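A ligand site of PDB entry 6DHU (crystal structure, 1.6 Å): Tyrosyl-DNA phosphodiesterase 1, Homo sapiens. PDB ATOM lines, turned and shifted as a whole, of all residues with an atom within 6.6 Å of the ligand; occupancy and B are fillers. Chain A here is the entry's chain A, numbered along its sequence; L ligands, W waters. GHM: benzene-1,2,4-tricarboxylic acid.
NZ of Lys 118 is in salt-bridge range of O3 of the ligand (2.6 Å).
The side-chain amino group (NZ) of Lys 348 lies within salt-bridge range of an oxygen (O5) of the ligand, 2.6 Å away.
O6 of the ligand is in hydrogen-bond range of OG of Ser 252 (2.6 Å).
The side-chain amide nitrogen (ND2) of Asn 136 sits at hydrogen-bond distance from an oxygen (O4) of the ligand (2.7 Å).
O4 of the ligand sits at hydrogen-bond distance from NE2 of His 346, 2.7 Å away.
A ring nitrogen (ND1) of His 116 is in hydrogen-bond range of an oxygen (O3) of the ligand, 3.1 Å away.
ND2 of Asn 369 lies close to O6 of the ligand, 3.2 Å away.
The side-chain hydroxyl (OG) of Ser 253 sits at hydrogen-bond distance from an oxygen (O1) of the ligand (3.4 Å).
NZ of Lys 118 is in hydrogen-bond range of O of His 116, 2.8 Å away.
The side-chain amino group (NZ) of Lys 348 is in hydrogen-bond range of the side-chain hydroxyl (OG) of Ser 252.
The side-chain amino group (NZ) of Lys 348 sits at hydrogen-bond distance from the backbone carbonyl oxygen (O) of His 346 (2.8 Å).
The side-chain amide oxygen (OD1) of Asn 369 is in hydrogen-bond range of the backbone NH (N) of Ser 252.
The side-chain carboxylate of Asp 141 sits at hydrogen-bond distance from the backbone NH of Asn 136 (2.8 Å).
OD1 of Asn 136 sits close to OD1 of Asn 56, at 3.2 Å.
The backbone NH of Ser 253 is in hydrogen-bond range of the side-chain amide oxygen of Asn 369 (3.1 Å).
The side-chain hydroxyl of Ser 253 lies within hydrogen-bond range of the backbone carbonyl oxygen of Pro 314, at 3.4 Å.
Merely in contact with the ligand: Tyr 57 (3.3 Å) and Pro 314 (3.5 Å).
Hydrophobic or aromatic side chains within 4 Å of the ligand: Tyr 57, His 116, Pro 314 and His 346.
Within 4 Å of the ligand: Tyr 57, His 116, Lys 118, Asn 136, Ser 252, Ser 253, Pro 314, His 346, Lys 348 and Asn 369.
Water W1 lies within hydrogen-bond range of an oxygen (O5) of the ligand (2.6 Å), a ring nitrogen (ND1) of His 116 (2.9 Å), the backbone carbonyl oxygen of Ser 367 (2.9 Å) and the side-chain amino group of Lys 118 (3.4 Å).
Water W2 bridges ND2 of Asn 369 and NE2 of His 116.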
ATOM      1  N   ASN A  56     -19.460 -13.428  -3.716  1.00  0.00           N
ATOM      2  CA  ASN A  56     -18.855 -13.150  -2.431  1.00  0.00           C
ATOM      3  C   ASN A  56     -17.459 -12.600  -2.596  1.00  0.00           C
ATOM      4  O   ASN A  56     -16.974 -12.375  -3.718  1.00  0.00           O
ATOM      5  CB  ASN A  56     -18.850 -14.396  -1.529  1.00  0.00           C
ATOM      6  CG  ASN A  56     -19.188 -14.045  -0.086  1.00  0.00           C
ATOM      7  OD1 ASN A  56     -18.396 -13.407   0.579  1.00  0.00           O
ATOM      8  ND2 ASN A  56     -20.386 -14.416   0.381  1.00  0.00           N
ATOM      9  N   TYR A  57     -16.801 -12.389  -1.457  1.00  0.00           N
ATOM     10  CA  TYR A  57     -15.430 -11.942  -1.386  1.00  0.00           C
ATOM     11  C   TYR A  57     -14.484 -13.099  -1.077  1.00  0.00           C
ATOM     12  O   TYR A  57     -13.564 -13.387  -1.851  1.00  0.00           O
ATOM     13  CB  TYR A  57     -15.313 -10.848  -0.318  1.00  0.00           C
ATOM     14  CG  TYR A  57     -13.884 -10.423  -0.088  1.00  0.00           C
ATOM     15  CD1 TYR A  57     -13.189  -9.714  -1.056  1.00  0.00           C
ATOM     16  CD2 TYR A  57     -13.232 -10.743   1.097  1.00  0.00           C
ATOM     17  CE1 TYR A  57     -11.875  -9.335  -0.846  1.00  0.00           C
ATOM     18  CE2 TYR A  57     -11.915 -10.380   1.303  1.00  0.00           C
ATOM     19  CZ  TYR A  57     -11.249  -9.670   0.335  1.00  0.00           C
ATOM     20  OH  TYR A  57      -9.939  -9.300   0.559  1.00  0.00           O
ATOM     21  N   CYS A  58     -14.711 -13.793   0.054  1.00  0.00           N
ATOM     22  CA  CYS A  58     -13.862 -14.883   0.506  1.00  0.00           C
ATOM     23  C   CYS A  58     -14.638 -16.194   0.516  1.00  0.00           C
ATOM     24  O   CYS A  58     -15.765 -16.240   1.021  1.00  0.00           O
ATOM     25  CB  CYS A  58     -13.309 -14.597   1.908  1.00  0.00           C
ATOM     26  SG  CYS A  58     -12.007 -15.736   2.431  1.00  0.00           S
ATOM     27  N   THR A 114     -12.543  -3.929  -4.824  1.00  0.00           N
ATOM     28  CA  THR A 114     -12.754  -5.320  -4.445  1.00  0.00           C
ATOM     29  C   THR A 114     -14.193  -5.701  -4.733  1.00  0.00           C
ATOM     30  O   THR A 114     -15.088  -4.865  -4.771  1.00  0.00           O
ATOM     31  CB  THR A 114     -12.473  -5.568  -2.953  1.00  0.00           C
ATOM     32  OG1 THR A 114     -13.177  -4.586  -2.177  1.00  0.00           O
ATOM     33  CG2 THR A 114     -10.992  -5.532  -2.652  1.00  0.00           C
ATOM     34  N   HIS A 115     -14.397  -7.008  -4.888  1.00  0.00           N
ATOM     35  CA  HIS A 115     -15.740  -7.568  -5.105  1.00  0.00           C
ATOM     36  C   HIS A 115     -16.305  -7.954  -3.741  1.00  0.00           C
ATOM     37  O   HIS A 115     -16.073  -9.060  -3.239  1.00  0.00           O
ATOM     38  CB  HIS A 115     -15.698  -8.757  -6.049  1.00  0.00           C
ATOM     39  CG  HIS A 115     -17.058  -9.286  -6.368  1.00  0.00           C
ATOM     40  ND1 HIS A 115     -17.639 -10.329  -5.669  1.00  0.00           N
ATOM     41  CD2 HIS A 115     -17.972  -8.894  -7.287  1.00  0.00           C
ATOM     42  CE1 HIS A 115     -18.845 -10.567  -6.159  1.00  0.00           C
ATOM     43  NE2 HIS A 115     -19.079  -9.707  -7.139  1.00  0.00           N
ATOM     44  N   HIS A 116     -17.078  -7.037  -3.146  1.00  0.00           N
ATOM     45  CA  HIS A 116     -17.584  -7.216  -1.786  1.00  0.00           C
ATOM     46  C   HIS A 116     -19.007  -7.780  -1.740  1.00  0.00           C
ATOM     47  O   HIS A 116     -19.415  -8.267  -0.678  1.00  0.00           O
ATOM     48  CB  HIS A 116     -17.616  -5.890  -1.018  1.00  0.00           C
ATOM     49  CG  HIS A 116     -16.307  -5.477  -0.444  1.00  0.00           C
ATOM     50  ND1 HIS A 116     -15.650  -6.215   0.519  1.00  0.00           N
ATOM     51  CD2 HIS A 116     -15.562  -4.366  -0.640  1.00  0.00           C
ATOM     52  CE1 HIS A 116     -14.530  -5.593   0.858  1.00  0.00           C
ATOM     53  NE2 HIS A 116     -14.460  -4.465   0.166  1.00  0.00           N
ATOM     54  N   THR A 117     -19.752  -7.681  -2.833  1.00  0.00           N
ATOM     55  CA  THR A 117     -21.144  -8.122  -2.891  1.00  0.00           C
ATOM     56  C   THR A 117     -21.312  -9.555  -2.395  1.00  0.00           C
ATOM     57  O   THR A 117     -20.569 -10.460  -2.775  1.00  0.00           O
ATOM     58  CB  THR A 117     -21.611  -8.008  -4.331  1.00  0.00           C
ATOM     59  OG1 THR A 117     -21.723  -6.622  -4.652  1.00  0.00           O
ATOM     60  CG2 THR A 117     -22.976  -8.728  -4.540  1.00  0.00           C
ATOM     61  N   LYS A 118     -22.316  -9.759  -1.530  1.00  0.00           N
ATOM     62  CA  LYS A 118     -22.629 -11.057  -0.951  1.00  0.00           C
ATOM     63  C   LYS A 118     -24.089 -11.368  -1.291  1.00  0.00           C
ATOM     64  O   LYS A 118     -25.022 -10.724  -0.779  1.00  0.00           O
ATOM     65  CB  LYS A 118     -22.341 -11.049   0.541  1.00  0.00           C
ATOM     66  CG  LYS A 118     -20.822 -10.840   0.729  1.00  0.00           C
ATOM     67  CD  LYS A 118     -20.392 -10.754   2.145  1.00  0.00           C
ATOM     68  CE  LYS A 118     -18.910 -10.511   2.199  1.00  0.00           C
ATOM     69  NZ  LYS A 118     -18.582  -9.120   1.827  1.00  0.00           N
ATOM     70  N   THR A 134     -24.541 -10.501   4.290  1.00  0.00           N
ATOM     71  CA  THR A 134     -23.300  -9.814   4.644  1.00  0.00           C
ATOM     72  C   THR A 134     -22.144 -10.754   4.964  1.00  0.00           C
ATOM     73  O   THR A 134     -21.036 -10.265   5.268  1.00  0.00           O
ATOM     74  CB  THR A 134     -23.506  -8.855   5.843  1.00  0.00           C
ATOM     75  OG1 THR A 134     -23.882  -9.566   7.032  1.00  0.00           O
ATOM     76  CG2 THR A 134     -24.575  -7.815   5.543  1.00  0.00           C
ATOM     77  N   SER A 135     -22.315 -12.072   4.873  1.00  0.00           N
ATOM     78  CA  SER A 135     -21.298 -13.017   5.330  1.00  0.00           C
ATOM     79  C   SER A 135     -20.428 -13.546   4.208  1.00  0.00           C
ATOM     80  O   SER A 135     -20.919 -13.882   3.130  1.00  0.00           O
ATOM     81  CB  SER A 135     -21.947 -14.216   6.041  1.00  0.00           C
ATOM     82  OG  SER A 135     -22.785 -13.833   7.115  1.00  0.00           O
ATOM     83  N   ASN A 136     -19.135 -13.667   4.478  1.00  0.00           N
ATOM     84  CA  ASN A 136     -18.249 -14.431   3.610  1.00  0.00           C
ATOM     85  C   ASN A 136     -18.600 -15.917   3.704  1.00  0.00           C
ATOM     86  O   ASN A 136     -19.231 -16.369   4.658  1.00  0.00           O
ATOM     87  CB  ASN A 136     -16.785 -14.216   3.996  1.00  0.00           C
ATOM     88  CG  ASN A 136     -16.319 -12.809   3.701  1.00  0.00           C
ATOM     89  OD1 ASN A 136     -15.994 -12.475   2.552  1.00  0.00           O
ATOM     90  ND2 ASN A 136     -16.300 -11.961   4.720  1.00  0.00           N
ATOM     91  N   ASP A 141     -17.473 -16.749   9.530  1.00  0.00           N
ATOM     92  CA  ASP A 141     -18.436 -15.673   9.333  1.00  0.00           C
ATOM     93  C   ASP A 141     -19.848 -16.056   9.728  1.00  0.00           C
ATOM     94  O   ASP A 141     -20.690 -15.174   9.932  1.00  0.00           O
ATOM     95  CB  ASP A 141     -18.417 -15.208   7.873  1.00  0.00           C
ATOM     96  CG  ASP A 141     -17.519 -14.007   7.680  1.00  0.00           C
ATOM     97  OD1 ASP A 141     -16.441 -13.976   8.323  1.00  0.00           O
ATOM     98  OD2 ASP A 141     -17.886 -13.080   6.910  1.00  0.00           O
ATOM     99  N   PHE A 251     -20.738  -0.349  10.750  1.00  0.00           N
ATOM    100  CA  PHE A 251     -19.882  -0.950   9.726  1.00  0.00           C
ATOM    101  C   PHE A 251     -18.752  -1.731  10.380  1.00  0.00           C
ATOM    102  O   PHE A 251     -18.534  -1.647  11.592  1.00  0.00           O
ATOM    103  CB  PHE A 251     -19.315   0.137   8.815  1.00  0.00           C
ATOM    104  CG  PHE A 251     -18.858   1.343   9.584  1.00  0.00           C
ATOM    105  CD1 PHE A 251     -17.618   1.340  10.198  1.00  0.00           C
ATOM    106  CD2 PHE A 251     -19.714   2.431   9.780  1.00  0.00           C
ATOM    107  CE1 PHE A 251     -17.201   2.417  10.954  1.00  0.00           C
ATOM    108  CE2 PHE A 251     -19.304   3.501  10.537  1.00  0.00           C
ATOM    109  CZ  PHE A 251     -18.044   3.505  11.132  1.00  0.00           C
ATOM    110  N   SER A 252     -18.009  -2.479   9.557  1.00  0.00           N
ATOM    111  CA  SER A 252     -16.935  -3.334  10.063  1.00  0.00           C
ATOM    112  C   SER A 252     -15.564  -2.910   9.565  1.00  0.00           C
ATOM    113  O   SER A 252     -14.562  -3.561   9.916  1.00  0.00           O
ATOM    114  CB  SER A 252     -17.203  -4.799   9.691  1.00  0.00           C
ATOM    115  OG  SER A 252     -17.206  -4.999   8.287  1.00  0.00           O
ATOM    116  N   SER A 253     -15.477  -1.866   8.755  1.00  0.00           N
ATOM    117  CA  SER A 253     -14.194  -1.306   8.348  1.00  0.00           C
ATOM    118  C   SER A 253     -14.425   0.142   7.933  1.00  0.00           C
ATOM    119  O   SER A 253     -15.546   0.554   7.649  1.00  0.00           O
ATOM    120  CB  SER A 253     -13.548  -2.095   7.207  1.00  0.00           C
ATOM    121  OG  SER A 253     -12.188  -1.740   7.108  1.00  0.00           O
ATOM    122  N   VAL A 254     -13.332   0.900   7.921  1.00  0.00           N
ATOM    123  CA  VAL A 254     -13.343   2.311   7.556  1.00  0.00           C
ATOM    124  C   VAL A 254     -12.212   2.533   6.565  1.00  0.00           C
ATOM    125  O   VAL A 254     -11.098   2.034   6.759  1.00  0.00           O
ATOM    126  CB  VAL A 254     -13.150   3.238   8.775  1.00  0.00           C
ATOM    127  CG1 VAL A 254     -13.578   4.645   8.411  1.00  0.00           C
ATOM    128  CG2 VAL A 254     -13.893   2.716   9.999  1.00  0.00           C
ATOM    129  N   SER A 312     -11.585  -9.712  11.261  1.00  0.00           N
ATOM    130  CA  SER A 312     -12.667  -9.339  10.360  1.00  0.00           C
ATOM    131  C   SER A 312     -13.122  -7.896  10.572  1.00  0.00           C
ATOM    132  O   SER A 312     -14.219  -7.525  10.130  1.00  0.00           O
ATOM    133  CB  SER A 312     -13.844 -10.292  10.523  1.00  0.00           C
ATOM    134  OG  SER A 312     -13.450 -11.620  10.200  1.00  0.00           O
ATOM    135  N   LEU A 313     -12.291  -7.089  11.220  1.00  0.00           N
ATOM    136  CA  LEU A 313     -12.546  -5.658  11.418  1.00  0.00           C
ATOM    137  C   LEU A 313     -11.281  -4.933  10.963  1.00  0.00           C
ATOM    138  O   LEU A 313     -10.485  -4.449  11.770  1.00  0.00           O
ATOM    139  CB  LEU A 313     -12.863  -5.367  12.885  1.00  0.00           C
ATOM    140  CG  LEU A 313     -14.156  -5.967  13.458  1.00  0.00           C
ATOM    141  CD1 LEU A 313     -14.144  -5.995  14.994  1.00  0.00           C
ATOM    142  CD2 LEU A 313     -15.389  -5.226  12.935  1.00  0.00           C
ATOM    143  N   PRO A 314     -11.049  -4.864   9.635  1.00  0.00           N
ATOM    144  CA  PRO A 314      -9.714  -4.548   9.104  1.00  0.00           C
ATOM    145  C   PRO A 314      -9.384  -3.061   8.978  1.00  0.00           C
ATOM    146  O   PRO A 314      -8.951  -2.599   7.914  1.00  0.00           O
ATOM    147  CB  PRO A 314      -9.712  -5.248   7.746  1.00  0.00           C
ATOM    148  CG  PRO A 314     -11.140  -5.238   7.328  1.00  0.00           C
ATOM    149  CD  PRO A 314     -11.974  -5.311   8.578  1.00  0.00           C
ATOM    150  N   TYR A 315      -9.548  -2.321  10.073  1.00  0.00           N
ATOM    151  CA  TYR A 315      -9.152  -0.916  10.149  1.00  0.00           C
ATOM    152  C   TYR A 315      -7.668  -0.834  10.498  1.00  0.00           C
ATOM    153  O   TYR A 315      -7.250  -1.275  11.572  1.00  0.00           O
ATOM    154  CB  TYR A 315      -9.994  -0.225  11.217  1.00  0.00           C
ATOM    155  CG  TYR A 315      -9.969   1.280  11.251  1.00  0.00           C
ATOM    156  CD1 TYR A 315      -9.574   2.023  10.135  1.00  0.00           C
ATOM    157  CD2 TYR A 315     -10.370   1.974  12.385  1.00  0.00           C
ATOM    158  CE1 TYR A 315      -9.585   3.410  10.163  1.00  0.00           C
ATOM    159  CE2 TYR A 315     -10.382   3.361  12.413  1.00  0.00           C
ATOM    160  CZ  TYR A 315      -9.984   4.075  11.301  1.00  0.00           C
ATOM    161  OH  TYR A 315      -9.993   5.458  11.320  1.00  0.00           O
ATOM    162  N   HIS A 346     -20.287  -8.061  11.573  1.00  0.00           N
ATOM    163  CA  HIS A 346     -19.834  -7.972  10.200  1.00  0.00           C
ATOM    164  C   HIS A 346     -20.957  -7.520   9.283  1.00  0.00           C
ATOM    165  O   HIS A 346     -20.704  -7.246   8.100  1.00  0.00           O
ATOM    166  CB  HIS A 346     -19.256  -9.335   9.775  1.00  0.00           C
ATOM    167  CG  HIS A 346     -18.562  -9.332   8.449  1.00  0.00           C
ATOM    168  ND1 HIS A 346     -19.202  -9.702   7.286  1.00  0.00           N
ATOM    169  CD2 HIS A 346     -17.292  -9.016   8.103  1.00  0.00           C
ATOM    170  CE1 HIS A 346     -18.355  -9.600   6.271  1.00  0.00           C
ATOM    171  NE2 HIS A 346     -17.191  -9.200   6.740  1.00  0.00           N
ATOM    172  N   LYS A 348     -23.387  -4.583   7.915  1.00  0.00           N
ATOM    173  CA  LYS A 348     -23.298  -3.130   7.787  1.00  0.00           C
ATOM    174  C   LYS A 348     -24.722  -2.622   7.628  1.00  0.00           C
ATOM    175  O   LYS A 348     -25.491  -3.211   6.866  1.00  0.00           O
ATOM    176  CB  LYS A 348     -22.456  -2.671   6.582  1.00  0.00           C
ATOM    177  CG  LYS A 348     -20.989  -3.112   6.600  1.00  0.00           C
ATOM    178  CD  LYS A 348     -20.839  -4.512   6.036  1.00  0.00           C
ATOM    179  CE  LYS A 348     -19.370  -4.817   5.805  1.00  0.00           C
ATOM    180  NZ  LYS A 348     -19.042  -6.216   6.129  1.00  0.00           N
ATOM    181  N   SER A 367     -23.455  -4.669   2.040  1.00  0.00           N
ATOM    182  CA  SER A 367     -22.047  -5.026   2.170  1.00  0.00           C
ATOM    183  C   SER A 367     -21.152  -3.798   2.311  1.00  0.00           C
ATOM    184  O   SER A 367     -19.963  -3.949   2.662  1.00  0.00           O
ATOM    185  CB  SER A 367     -21.598  -5.859   0.955  1.00  0.00           C
ATOM    186  OG  SER A 367     -21.760  -5.106  -0.240  1.00  0.00           O
ATOM    187  N   ASN A 369     -19.028  -0.858   3.523  1.00  0.00           N
ATOM    188  CA  ASN A 369     -18.411  -0.257   4.699  1.00  0.00           C
ATOM    189  C   ASN A 369     -18.334   1.259   4.537  1.00  0.00           C
ATOM    190  O   ASN A 369     -18.780   1.832   3.531  1.00  0.00           O
ATOM    191  CB  ASN A 369     -17.023  -0.863   4.914  1.00  0.00           C
ATOM    192  CG  ASN A 369     -17.100  -2.140   5.707  1.00  0.00           C
ATOM    193  OD1 ASN A 369     -17.822  -2.210   6.695  1.00  0.00           O
ATOM    194  ND2 ASN A 369     -16.361  -3.159   5.263  1.00  0.00           N
HETATM  195  C4  GHM L   1     -13.186  -7.691   2.801  1.00  0.00           C
HETATM  196  C5  GHM L   1     -14.322  -7.545   3.574  1.00  0.00           C
HETATM  197  C6  GHM L   1     -15.457  -8.569   3.460  1.00  0.00           C
HETATM  198  C7  GHM L   1     -14.424  -6.461   4.439  1.00  0.00           C
HETATM  199  C8  GHM L   1     -15.667  -6.269   5.326  1.00  0.00           C
HETATM  200  C9  GHM L   1     -13.402  -5.540   4.525  1.00  0.00           C
HETATM  201  C3  GHM L   1     -12.154  -6.767   2.877  1.00  0.00           C
HETATM  202  C1  GHM L   1     -11.158  -4.665   3.857  1.00  0.00           C
HETATM  203  C2  GHM L   1     -12.270  -5.697   3.744  1.00  0.00           C
HETATM  204  O1  GHM L   1     -11.419  -3.518   4.300  1.00  0.00           O
HETATM  205  O2  GHM L   1      -9.990  -4.972   3.518  1.00  0.00           O
HETATM  206  O3  GHM L   1     -16.107  -8.642   2.388  1.00  0.00           O
HETATM  207  O4  GHM L   1     -15.734  -9.332   4.419  1.00  0.00           O
HETATM  208  O5  GHM L   1     -16.807  -6.417   4.830  1.00  0.00           O
HETATM  209  O6  GHM L   1     -15.549  -5.977   6.544  1.00  0.00           O
HETATM  210  O   HOH W   1     -17.796  -5.917   2.431  1.00  0.00           O
HETATM  211  O   HOH W   2     -14.814  -3.184   2.925  1.00  0.00           O
